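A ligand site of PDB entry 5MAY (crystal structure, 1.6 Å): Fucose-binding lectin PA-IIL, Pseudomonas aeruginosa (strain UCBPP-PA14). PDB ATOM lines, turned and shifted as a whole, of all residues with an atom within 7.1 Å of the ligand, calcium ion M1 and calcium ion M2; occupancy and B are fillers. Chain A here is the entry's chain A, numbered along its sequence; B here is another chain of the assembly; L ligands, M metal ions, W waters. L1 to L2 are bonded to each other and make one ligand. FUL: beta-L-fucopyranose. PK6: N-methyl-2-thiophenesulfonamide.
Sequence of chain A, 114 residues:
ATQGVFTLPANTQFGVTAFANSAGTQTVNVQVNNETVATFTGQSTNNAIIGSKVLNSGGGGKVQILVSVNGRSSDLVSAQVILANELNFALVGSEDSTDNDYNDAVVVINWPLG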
ATOM      1  N   ALA A  20      14.338 -13.442  -0.298  1.00  0.00           N
ATOM      2  CA  ALA A  20      13.789 -13.854   1.014  1.00  0.00           C
ATOM      3  C   ALA A  20      12.572 -14.717   0.863  1.00  0.00           C
ATOM      4  O   ALA A  20      11.744 -14.520  -0.034  1.00  0.00           O
ATOM      5  CB  ALA A  20      13.444 -12.646   1.874  1.00  0.00           C
ATOM      6  N   ASN A  21      12.494 -15.732   1.720  1.00  0.00           N
ATOM      7  CA  ASN A  21      11.366 -16.681   1.770  1.00  0.00           C
ATOM      8  C   ASN A  21      11.161 -17.119   3.225  1.00  0.00           C
ATOM      9  O   ASN A  21      11.427 -18.270   3.577  1.00  0.00           O
ATOM     10  CB  ASN A  21      11.650 -17.934   0.923  1.00  0.00           C
ATOM     11  CG  ASN A  21      11.680 -17.656  -0.556  1.00  0.00           C
ATOM     12  OD1 ASN A  21      10.634 -17.510  -1.210  1.00  0.00           O
ATOM     13  ND2 ASN A  21      12.873 -17.531  -1.104  1.00  0.00           N
ATOM     14  N   SER A  22      10.631 -16.204   4.041  1.00  0.00           N
ATOM     15  CA  SER A  22      10.470 -16.482   5.436  1.00  0.00           C
ATOM     16  C   SER A  22       9.528 -15.468   6.066  1.00  0.00           C
ATOM     17  O   SER A  22       9.471 -14.332   5.598  1.00  0.00           O
ATOM     18  CB  SER A  22      11.818 -16.385   6.119  1.00  0.00           C
ATOM     19  OG  SER A  22      11.691 -16.502   7.565  1.00  0.00           O
ATOM     20  N   ALA A  23       8.882 -15.869   7.149  1.00  0.00           N
ATOM     21  CA  ALA A  23       8.133 -14.873   7.938  1.00  0.00           C
ATOM     22  C   ALA A  23       9.072 -13.899   8.669  1.00  0.00           C
ATOM     23  O   ALA A  23       8.644 -12.784   9.007  1.00  0.00           O
ATOM     24  CB  ALA A  23       7.239 -15.570   8.950  1.00  0.00           C
ATOM     25  N   GLY A  24      10.314 -14.295   8.899  1.00  0.00           N
ATOM     26  CA  GLY A  24      11.304 -13.469   9.590  1.00  0.00           C
ATOM     27  C   GLY A  24      11.986 -12.457   8.714  1.00  0.00           C
ATOM     28  O   GLY A  24      12.256 -12.736   7.542  1.00  0.00           O
ATOM     29  N   THR A  25      12.298 -11.310   9.275  1.00  0.00           N
ATOM     30  CA  THR A  25      13.059 -10.289   8.564  1.00  0.00           C
ATOM     31  C   THR A  25      14.488 -10.761   8.462  1.00  0.00           C
ATOM     32  O   THR A  25      15.113 -11.042   9.490  1.00  0.00           O
ATOM     33  CB  THR A  25      12.973  -8.943   9.280  1.00  0.00           C
ATOM     34  OG1 THR A  25      11.595  -8.544   9.224  1.00  0.00           O
ATOM     35  CG2 THR A  25      13.808  -7.911   8.619  1.00  0.00           C
ATOM     36  N   GLN A  26      15.021 -10.836   7.245  1.00  0.00           N
ATOM     37  CA  GLN A  26      16.369 -11.329   7.008  1.00  0.00           C
ATOM     38  C   GLN A  26      17.366 -10.177   6.962  1.00  0.00           C
ATOM     39  O   GLN A  26      17.100  -9.161   6.301  1.00  0.00           O
ATOM     40  CB  GLN A  26      16.405 -12.041   5.666  1.00  0.00           C
ATOM     41  CG  GLN A  26      15.370 -13.137   5.480  1.00  0.00           C
ATOM     42  CD  GLN A  26      15.620 -14.305   6.425  1.00  0.00           C
ATOM     43  OE1 GLN A  26      16.711 -14.858   6.463  1.00  0.00           O
ATOM     44  NE2 GLN A  26      14.583 -14.711   7.135  1.00  0.00           N
ATOM     45  N   SER A  44      10.083 -11.275   2.926  1.00  0.00           N
ATOM     46  CA  SER A  44       9.199 -11.786   1.923  1.00  0.00           C
ATOM     47  C   SER A  44       8.981 -13.245   2.135  1.00  0.00           C
ATOM     48  O   SER A  44       9.913 -13.919   2.559  1.00  0.00           O
ATOM     49  CB  SER A  44       9.788 -11.564   0.524  1.00  0.00           C
ATOM     50  OG  SER A  44       8.943 -12.078  -0.522  1.00  0.00           O
ATOM     51  N   THR A  45       7.771 -13.730   1.890  1.00  0.00           N
ATOM     52  CA  THR A  45       7.530 -15.166   1.758  1.00  0.00           C
ATOM     53  C   THR A  45       7.333 -15.558   0.280  1.00  0.00           C
ATOM     54  O   THR A  45       6.917 -16.689   0.004  1.00  0.00           O
ATOM     55  CB  THR A  45       6.364 -15.660   2.596  1.00  0.00           C
ATOM     56  OG1 THR A  45       5.231 -14.804   2.292  1.00  0.00           O
ATOM     57  CG2 THR A  45       6.711 -15.576   4.057  1.00  0.00           C
ATOM     58  N   VAL A  69      18.541 -13.409  11.692  1.00  0.00           N
ATOM     59  CA  VAL A  69      17.127 -13.076  11.819  1.00  0.00           C
ATOM     60  C   VAL A  69      16.986 -12.771  13.323  1.00  0.00           C
ATOM     61  O   VAL A  69      17.307 -13.608  14.133  1.00  0.00           O
ATOM     62  CB  VAL A  69      16.234 -14.232  11.426  1.00  0.00           C
ATOM     63  CG1 VAL A  69      14.731 -13.874  11.646  1.00  0.00           C
ATOM     64  CG2 VAL A  69      16.481 -14.600   9.974  1.00  0.00           C
ATOM     65  N   ASN A  70      16.568 -11.572  13.618  1.00  0.00           N
ATOM     66  CA  ASN A  70      16.408 -11.146  15.024  1.00  0.00           C
ATOM     67  C   ASN A  70      17.679 -11.304  15.835  1.00  0.00           C
ATOM     68  O   ASN A  70      17.665 -11.791  16.972  1.00  0.00           O
ATOM     69  CB  ASN A  70      15.313 -11.968  15.700  1.00  0.00           C
ATOM     70  CG  ASN A  70      14.053 -11.204  15.781  1.00  0.00           C
ATOM     71  OD1 ASN A  70      13.158 -11.443  14.970  1.00  0.00           O
ATOM     72  ND2 ASN A  70      14.008 -10.180  16.680  1.00  0.00           N
ATOM     73  N   ARG A  72      19.853 -13.633  15.561  1.00  0.00           N
ATOM     74  CA  ARG A  72      20.303 -14.998  15.622  1.00  0.00           C
ATOM     75  C   ARG A  72      20.865 -15.423  14.273  1.00  0.00           C
ATOM     76  O   ARG A  72      20.193 -15.236  13.268  1.00  0.00           O
ATOM     77  CB  ARG A  72      19.152 -15.890  15.888  1.00  0.00           C
ATOM     78  CG  ARG A  72      19.488 -17.333  16.091  1.00  0.00           C
ATOM     79  CD  ARG A  72      18.151 -18.021  16.337  1.00  0.00           C
ATOM     80  NE  ARG A  72      18.271 -19.266  17.059  1.00  0.00           N
ATOM     81  CZ  ARG A  72      17.504 -19.646  18.104  1.00  0.00           C
ATOM     82  NH1 ARG A  72      16.561 -18.846  18.636  1.00  0.00           N
ATOM     83  NH2 ARG A  72      17.721 -20.847  18.647  1.00  0.00           N
ATOM     84  N   SER A  94      20.014 -20.518   3.559  1.00  0.00           N
ATOM     85  CA  SER A  94      20.068 -20.278   5.012  1.00  0.00           C
ATOM     86  C   SER A  94      18.748 -20.699   5.653  1.00  0.00           C
ATOM     87  O   SER A  94      17.719 -20.612   5.019  1.00  0.00           O
ATOM     88  CB  SER A  94      20.395 -18.830   5.279  1.00  0.00           C
ATOM     89  OG  SER A  94      19.362 -17.944   4.898  1.00  0.00           O
ATOM     90  N   GLU A  95      18.832 -21.124   6.911  1.00  0.00           N
ATOM     91  CA  GLU A  95      17.697 -21.664   7.649  1.00  0.00           C
ATOM     92  C   GLU A  95      17.641 -20.930   8.978  1.00  0.00           C
ATOM     93  O   GLU A  95      18.566 -21.021   9.773  1.00  0.00           O
ATOM     94  CB  GLU A  95      17.848 -23.153   7.887  1.00  0.00           C
ATOM     95  CG  GLU A  95      16.715 -23.746   8.684  1.00  0.00           C
ATOM     96  CD  GLU A  95      15.373 -23.476   8.101  1.00  0.00           C
ATOM     97  OE1 GLU A  95      15.152 -23.717   6.855  1.00  0.00           O
ATOM     98  OE2 GLU A  95      14.457 -22.934   8.858  1.00  0.00           O
ATOM     99  N   ASP A  96      16.509 -20.259   9.177  1.00  0.00           N
ATOM    100  CA  ASP A  96      16.282 -19.458  10.377  1.00  0.00           C
ATOM    101  C   ASP A  96      15.468 -20.175  11.448  1.00  0.00           C
ATOM    102  O   ASP A  96      15.288 -19.663  12.576  1.00  0.00           O
ATOM    103  CB  ASP A  96      15.701 -18.130  10.013  1.00  0.00           C
ATOM    104  CG  ASP A  96      14.330 -18.201   9.398  1.00  0.00           C
ATOM    105  OD1 ASP A  96      13.629 -19.235   9.546  1.00  0.00           O
ATOM    106  OD2 ASP A  96      13.980 -17.199   8.727  1.00  0.00           O
ATOM    107  N   SER A  97      15.044 -21.381  11.144  1.00  0.00           N
ATOM    108  CA  SER A  97      14.145 -22.146  12.027  1.00  0.00           C
ATOM    109  C   SER A  97      14.473 -23.616  11.896  1.00  0.00           C
ATOM    110  O   SER A  97      15.637 -23.981  11.872  1.00  0.00           O
ATOM    111  CB  SER A  97      12.711 -21.762  11.698  1.00  0.00           C
ATOM    112  OG  SER A  97      11.791 -22.355  12.588  1.00  0.00           O
ATOM    113  N   THR A  98      13.477 -24.495  11.880  1.00  0.00           N
ATOM    114  CA  THR A  98      13.688 -25.926  11.951  1.00  0.00           C
ATOM    115  C   THR A  98      12.889 -26.679  10.898  1.00  0.00           C
ATOM    116  O   THR A  98      12.908 -27.948  10.893  1.00  0.00           O
ATOM    117  CB  THR A  98      13.356 -26.448  13.400  1.00  0.00           C
ATOM    118  OG1 THR A  98      12.147 -25.865  13.800  1.00  0.00           O
ATOM    119  CG2 THR A  98      14.458 -26.057  14.386  1.00  0.00           C
ATOM    120  N   ASP A  99      12.217 -25.991   9.992  1.00  0.00           N
ATOM    121  CA  ASP A  99      11.597 -26.730   8.829  1.00  0.00           C
ATOM    122  C   ASP A  99      12.619 -27.208   7.773  1.00  0.00           C
ATOM    123  O   ASP A  99      12.290 -28.059   6.951  1.00  0.00           O
ATOM    124  CB  ASP A  99      10.439 -25.981   8.161  1.00  0.00           C
ATOM    125  CG  ASP A  99      10.852 -24.721   7.424  1.00  0.00           C
ATOM    126  OD1 ASP A  99      11.958 -24.211   7.728  1.00  0.00           O
ATOM    127  OD2 ASP A  99      10.054 -24.287   6.562  1.00  0.00           O
ATOM    128  N   ASN A 100      13.823 -26.660   7.784  1.00  0.00           N
ATOM    129  CA  ASN A 100      14.903 -27.069   6.932  1.00  0.00           C
ATOM    130  C   ASN A 100      14.599 -26.960   5.423  1.00  0.00           C
ATOM    131  O   ASN A 100      14.946 -27.861   4.636  1.00  0.00           O
ATOM    132  CB  ASN A 100      15.387 -28.486   7.317  1.00  0.00           C
ATOM    133  CG  ASN A 100      15.957 -28.486   8.713  1.00  0.00           C
ATOM    134  OD1 ASN A 100      16.296 -27.429   9.243  1.00  0.00           O
ATOM    135  ND2 ASN A 100      15.951 -29.633   9.381  1.00  0.00           N
ATOM    136  N   ASP A 101      13.961 -25.872   5.039  1.00  0.00           N
ATOM    137  CA  ASP A 101      13.840 -25.549   3.620  1.00  0.00           C
ATOM    138  C   ASP A 101      15.073 -24.802   3.075  1.00  0.00           C
ATOM    139  O   ASP A 101      15.305 -24.817   1.871  1.00  0.00           O
ATOM    140  CB  ASP A 101      12.512 -24.889   3.234  1.00  0.00           C
ATOM    141  CG  ASP A 101      12.236 -23.575   3.882  1.00  0.00           C
ATOM    142  OD1 ASP A 101      13.003 -23.116   4.771  1.00  0.00           O
ATOM    143  OD2 ASP A 101      11.173 -22.968   3.555  1.00  0.00           O
ATOM    144  N   TYR A 102      15.876 -24.218   3.961  1.00  0.00           N
ATOM    145  CA  TYR A 102      17.120 -23.524   3.569  1.00  0.00           C
ATOM    146  C   TYR A 102      16.970 -22.441   2.570  1.00  0.00           C
ATOM    147  O   TYR A 102      17.941 -22.034   1.927  1.00  0.00           O
ATOM    148  CB  TYR A 102      18.240 -24.536   3.189  1.00  0.00           C
ATOM    149  CG  TYR A 102      18.808 -25.205   4.422  1.00  0.00           C
ATOM    150  CD1 TYR A 102      19.772 -24.529   5.137  1.00  0.00           C
ATOM    151  CD2 TYR A 102      18.284 -26.369   4.932  1.00  0.00           C
ATOM    152  CE1 TYR A 102      20.276 -25.017   6.347  1.00  0.00           C
ATOM    153  CE2 TYR A 102      18.808 -26.879   6.156  1.00  0.00           C
ATOM    154  CZ  TYR A 102      19.759 -26.131   6.853  1.00  0.00           C
ATOM    155  OH  TYR A 102      20.349 -26.524   8.070  1.00  0.00           O
ATOM    156  N   ASN A 103      15.751 -21.864   2.431  1.00  0.00           N
ATOM    157  CA  ASN A 103      15.513 -20.816   1.481  1.00  0.00           C
ATOM    158  C   ASN A 103      15.175 -19.480   2.136  1.00  0.00           C
ATOM    159  O   ASN A 103      14.754 -18.564   1.472  1.00  0.00           O
ATOM    160  CB  ASN A 103      14.392 -21.203   0.553  1.00  0.00           C
ATOM    161  CG  ASN A 103      13.047 -21.128   1.265  1.00  0.00           C
ATOM    162  OD1 ASN A 103      13.013 -20.930   2.488  1.00  0.00           O
ATOM    163  ND2 ASN A 103      11.962 -21.331   0.544  1.00  0.00           N
ATOM    164  N   ASP A 104      15.392 -19.364   3.444  1.00  0.00           N
ATOM    165  CA  ASP A 104      14.839 -18.239   4.156  1.00  0.00           C
ATOM    166  C   ASP A 104      15.477 -16.936   3.714  1.00  0.00           C
ATOM    167  O   ASP A 104      14.790 -15.921   3.529  1.00  0.00           O
ATOM    168  CB  ASP A 104      14.999 -18.488   5.661  1.00  0.00           C
ATOM    169  CG  ASP A 104      14.235 -19.701   6.111  1.00  0.00           C
ATOM    170  OD1 ASP A 104      13.136 -19.992   5.577  1.00  0.00           O
ATOM    171  OD2 ASP A 104      14.711 -20.468   6.985  1.00  0.00           O
ATOM    172  N   ALA A 105      16.792 -16.959   3.545  1.00  0.00           N
ATOM    173  CA  ALA A 105      17.498 -16.004   2.661  1.00  0.00           C
ATOM    174  C   ALA A 105      18.339 -16.854   1.709  1.00  0.00           C
ATOM    175  O   ALA A 105      19.041 -17.775   2.152  1.00  0.00           O
ATOM    176  CB  ALA A 105      18.399 -15.051   3.402  1.00  0.00           C
ATOM    177  N   PRO B 112      12.777 -24.495  -3.346  1.00  0.00           N
ATOM    178  CA  PRO B 112      11.422 -24.009  -3.153  1.00  0.00           C
ATOM    179  C   PRO B 112      11.331 -22.594  -2.732  1.00  0.00           C
ATOM    180  O   PRO B 112      12.341 -21.987  -2.248  1.00  0.00           O
ATOM    181  CB  PRO B 112      10.905 -24.911  -2.034  1.00  0.00           C
ATOM    182  CG  PRO B 112      12.120 -25.112  -1.229  1.00  0.00           C
ATOM    183  CD  PRO B 112      13.252 -25.256  -2.183  1.00  0.00           C
ATOM    184  N   LEU B 113      10.113 -22.057  -2.791  1.00  0.00           N
ATOM    185  CA  LEU B 113       9.843 -20.724  -2.244  1.00  0.00           C
ATOM    186  C   LEU B 113       9.015 -20.857  -0.948  1.00  0.00           C
ATOM    187  O   LEU B 113       8.592 -21.949  -0.562  1.00  0.00           O
ATOM    188  CB  LEU B 113       9.067 -19.893  -3.247  1.00  0.00           C
ATOM    189  CG  LEU B 113       9.676 -19.764  -4.648  1.00  0.00           C
ATOM    190  CD1 LEU B 113       8.895 -18.752  -5.464  1.00  0.00           C
ATOM    191  CD2 LEU B 113      11.145 -19.383  -4.554  1.00  0.00           C
ATOM    192  N   GLY B 114       8.822 -19.737  -0.273  1.00  0.00           N
ATOM    193  CA  GLY B 114       7.923 -19.691   0.864  1.00  0.00           C
ATOM    194  C   GLY B 114       8.584 -19.930   2.223  1.00  0.00           C
ATOM    195  O   GLY B 114       9.741 -20.428   2.332  1.00  0.00           O
ATOM    196  OXT GLY B 114       7.959 -19.529   3.215  1.00  0.00           O
HETATM  197  C1  FUL L   1       9.770 -19.420   8.930  1.00  0.00           C
HETATM  198  C2  FUL L   1      10.778 -20.074   7.951  1.00  0.00           C
HETATM  199  O2  FUL L   1      11.889 -20.786   8.538  1.00  0.00           O
HETATM  200  C3  FUL L   1      10.033 -21.135   7.178  1.00  0.00           C
HETATM  201  O3  FUL L   1      10.830 -21.862   6.214  1.00  0.00           O
HETATM  202  C4  FUL L   1       8.840 -20.524   6.460  1.00  0.00           C
HETATM  203  O4  FUL L   1       9.357 -19.736   5.363  1.00  0.00           O
HETATM  204  C5  FUL L   1       7.972 -19.679   7.384  1.00  0.00           C
HETATM  205  C6  FUL L   1       6.876 -18.934   6.637  1.00  0.00           C
HETATM  206  O5  FUL L   1       8.778 -18.733   8.143  1.00  0.00           O
HETATM  207  O1  PK6 L   2      10.816 -16.053  11.522  1.00  0.00           O
HETATM  208  S1  PK6 L   2       9.925 -17.072  11.975  1.00  0.00           S
HETATM  209  O2  PK6 L   2       8.726 -16.573  12.598  1.00  0.00           O
HETATM  210  N1  PK6 L   2       9.430 -17.965  10.728  1.00  0.00           N
HETATM  211  C1  PK6 L   2      10.509 -18.490   9.868  1.00  0.00           C
HETATM  212  C2  PK6 L   2      10.756 -18.028  13.044  1.00  0.00           C
HETATM  213  C3  PK6 L   2      10.175 -18.983  13.907  1.00  0.00           C
HETATM  214  C4  PK6 L   2      11.223 -19.573  14.633  1.00  0.00           C
HETATM  215  C5  PK6 L   2      12.503 -19.058  14.361  1.00  0.00           C
HETATM  216  S2  PK6 L   2      12.473 -17.828  13.144  1.00  0.00           S
HETATM  217 CA    CA M   1      11.359 -20.578   4.135  1.00  0.00          CA
HETATM  218 CA    CA M   2      13.124 -22.268   7.006  1.00  0.00          CA
HETATM  219  O   HOH W   1      12.709 -19.086  17.812  1.00  0.00           O
HETATM  220  O   HOH W   2       7.238 -19.295  11.402  1.00  0.00           O
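Calcium ion M1 is bound by the side-chain amide oxygen (OD1) of Asn 103 (2.4 Å), the side-chain carboxylate (OD1) of Asp 104 (2.4 Å), the backbone carbonyl oxygen (O) of Asn 21 (2.4 Å), the chain-end carboxylate (O) of Gly 114 of chain B (2.4 Å), the side-chain carboxylate (OD2) of Asp 101 (2.5 Å), an oxygen (O4) of FUL L1 (2.5 Å) and an oxygen (O3) of FUL L1 (2.5 Å).
Calcium ion M1 has seven donor atoms within binding distance.
Slightly farther from calcium ion M1 lies OD1 of Asp 101 (3.1 Å).
The nearest printed residue that does not touch calcium ion M1 is Ser 22 (4.4 Å).
Residues that only touch the ligand: Ser 22 (3.3 Å) and Ser 97 (3.4 Å).
Of the 27 residues printed, 11 come within 4 Å of the ligand.
N of Asn 103 is in hydrogen-bond range of O of Ser 94, 3.5 Å away.
The backbone NH of Asp 96 lies close to the side-chain carboxylate of Asp 104 (2.8 Å).
O of Ser 94 is in hydrogen-bond range of N of Asp 104, 3.1 Å away.
N of Asn 21 lies close to O of Ser 44, 3.3 Å away.
OE1 of Glu 95 lies close to N of Asn 100 (3.4 Å).
The backbone NH (N) of Tyr 102 sits close to the side-chain carboxylate (OE1) of Glu 95 (3.0 Å).
The backbone NH (N) of Gly 24 is in hydrogen-bond range of the side-chain hydroxyl (OG) of Ser 22 (2.9 Å).
The side-chain amide nitrogen (NE2) of Gln 26 sits close to the side-chain hydroxyl (OG) of Ser 22 (3.4 Å).
The side-chain carboxylate (OE2) of Glu 95 binds calcium ion M2, at 2.4 Å.
OD1 of Asp 99 binds calcium ion M2, 2.4 Å away.
OD1 of Asp 101 is bound to calcium ion M2 (2.4 Å).
Calcium ion M2 is bound by the side-chain carboxylate (OD2) of Asp 104 (2.4 Å).
Calcium ion M2 is bound by O3 of FUL L1.
An oxygen (O2) of FUL L1 binds calcium ion M2, at 2.5 Å.
The side-chain carboxylate (OE1) of Glu 95 binds calcium ion M2 (2.5 Å).
OD1 of Asp 104 is bound to calcium ion M2 (2.7 Å).
OD1 of Asp 96 touches calcium ion M2, at 3.99 Å.
Of the 27 residues printed, 5 come within 4 Å of calcium ion M2.
The nearest printed residue that does not touch calcium ion M2 is Asn 100 (4.5 Å).
OD1 of Asp 96 lies close to O2 of FUL L1 (2.5 Å).
N of Ala 23 sits at hydrogen-bond distance from O5 of FUL L1, at 3.0 Å.
O1 of PK6 L2 is in hydrogen-bond range of N of Gly 24.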
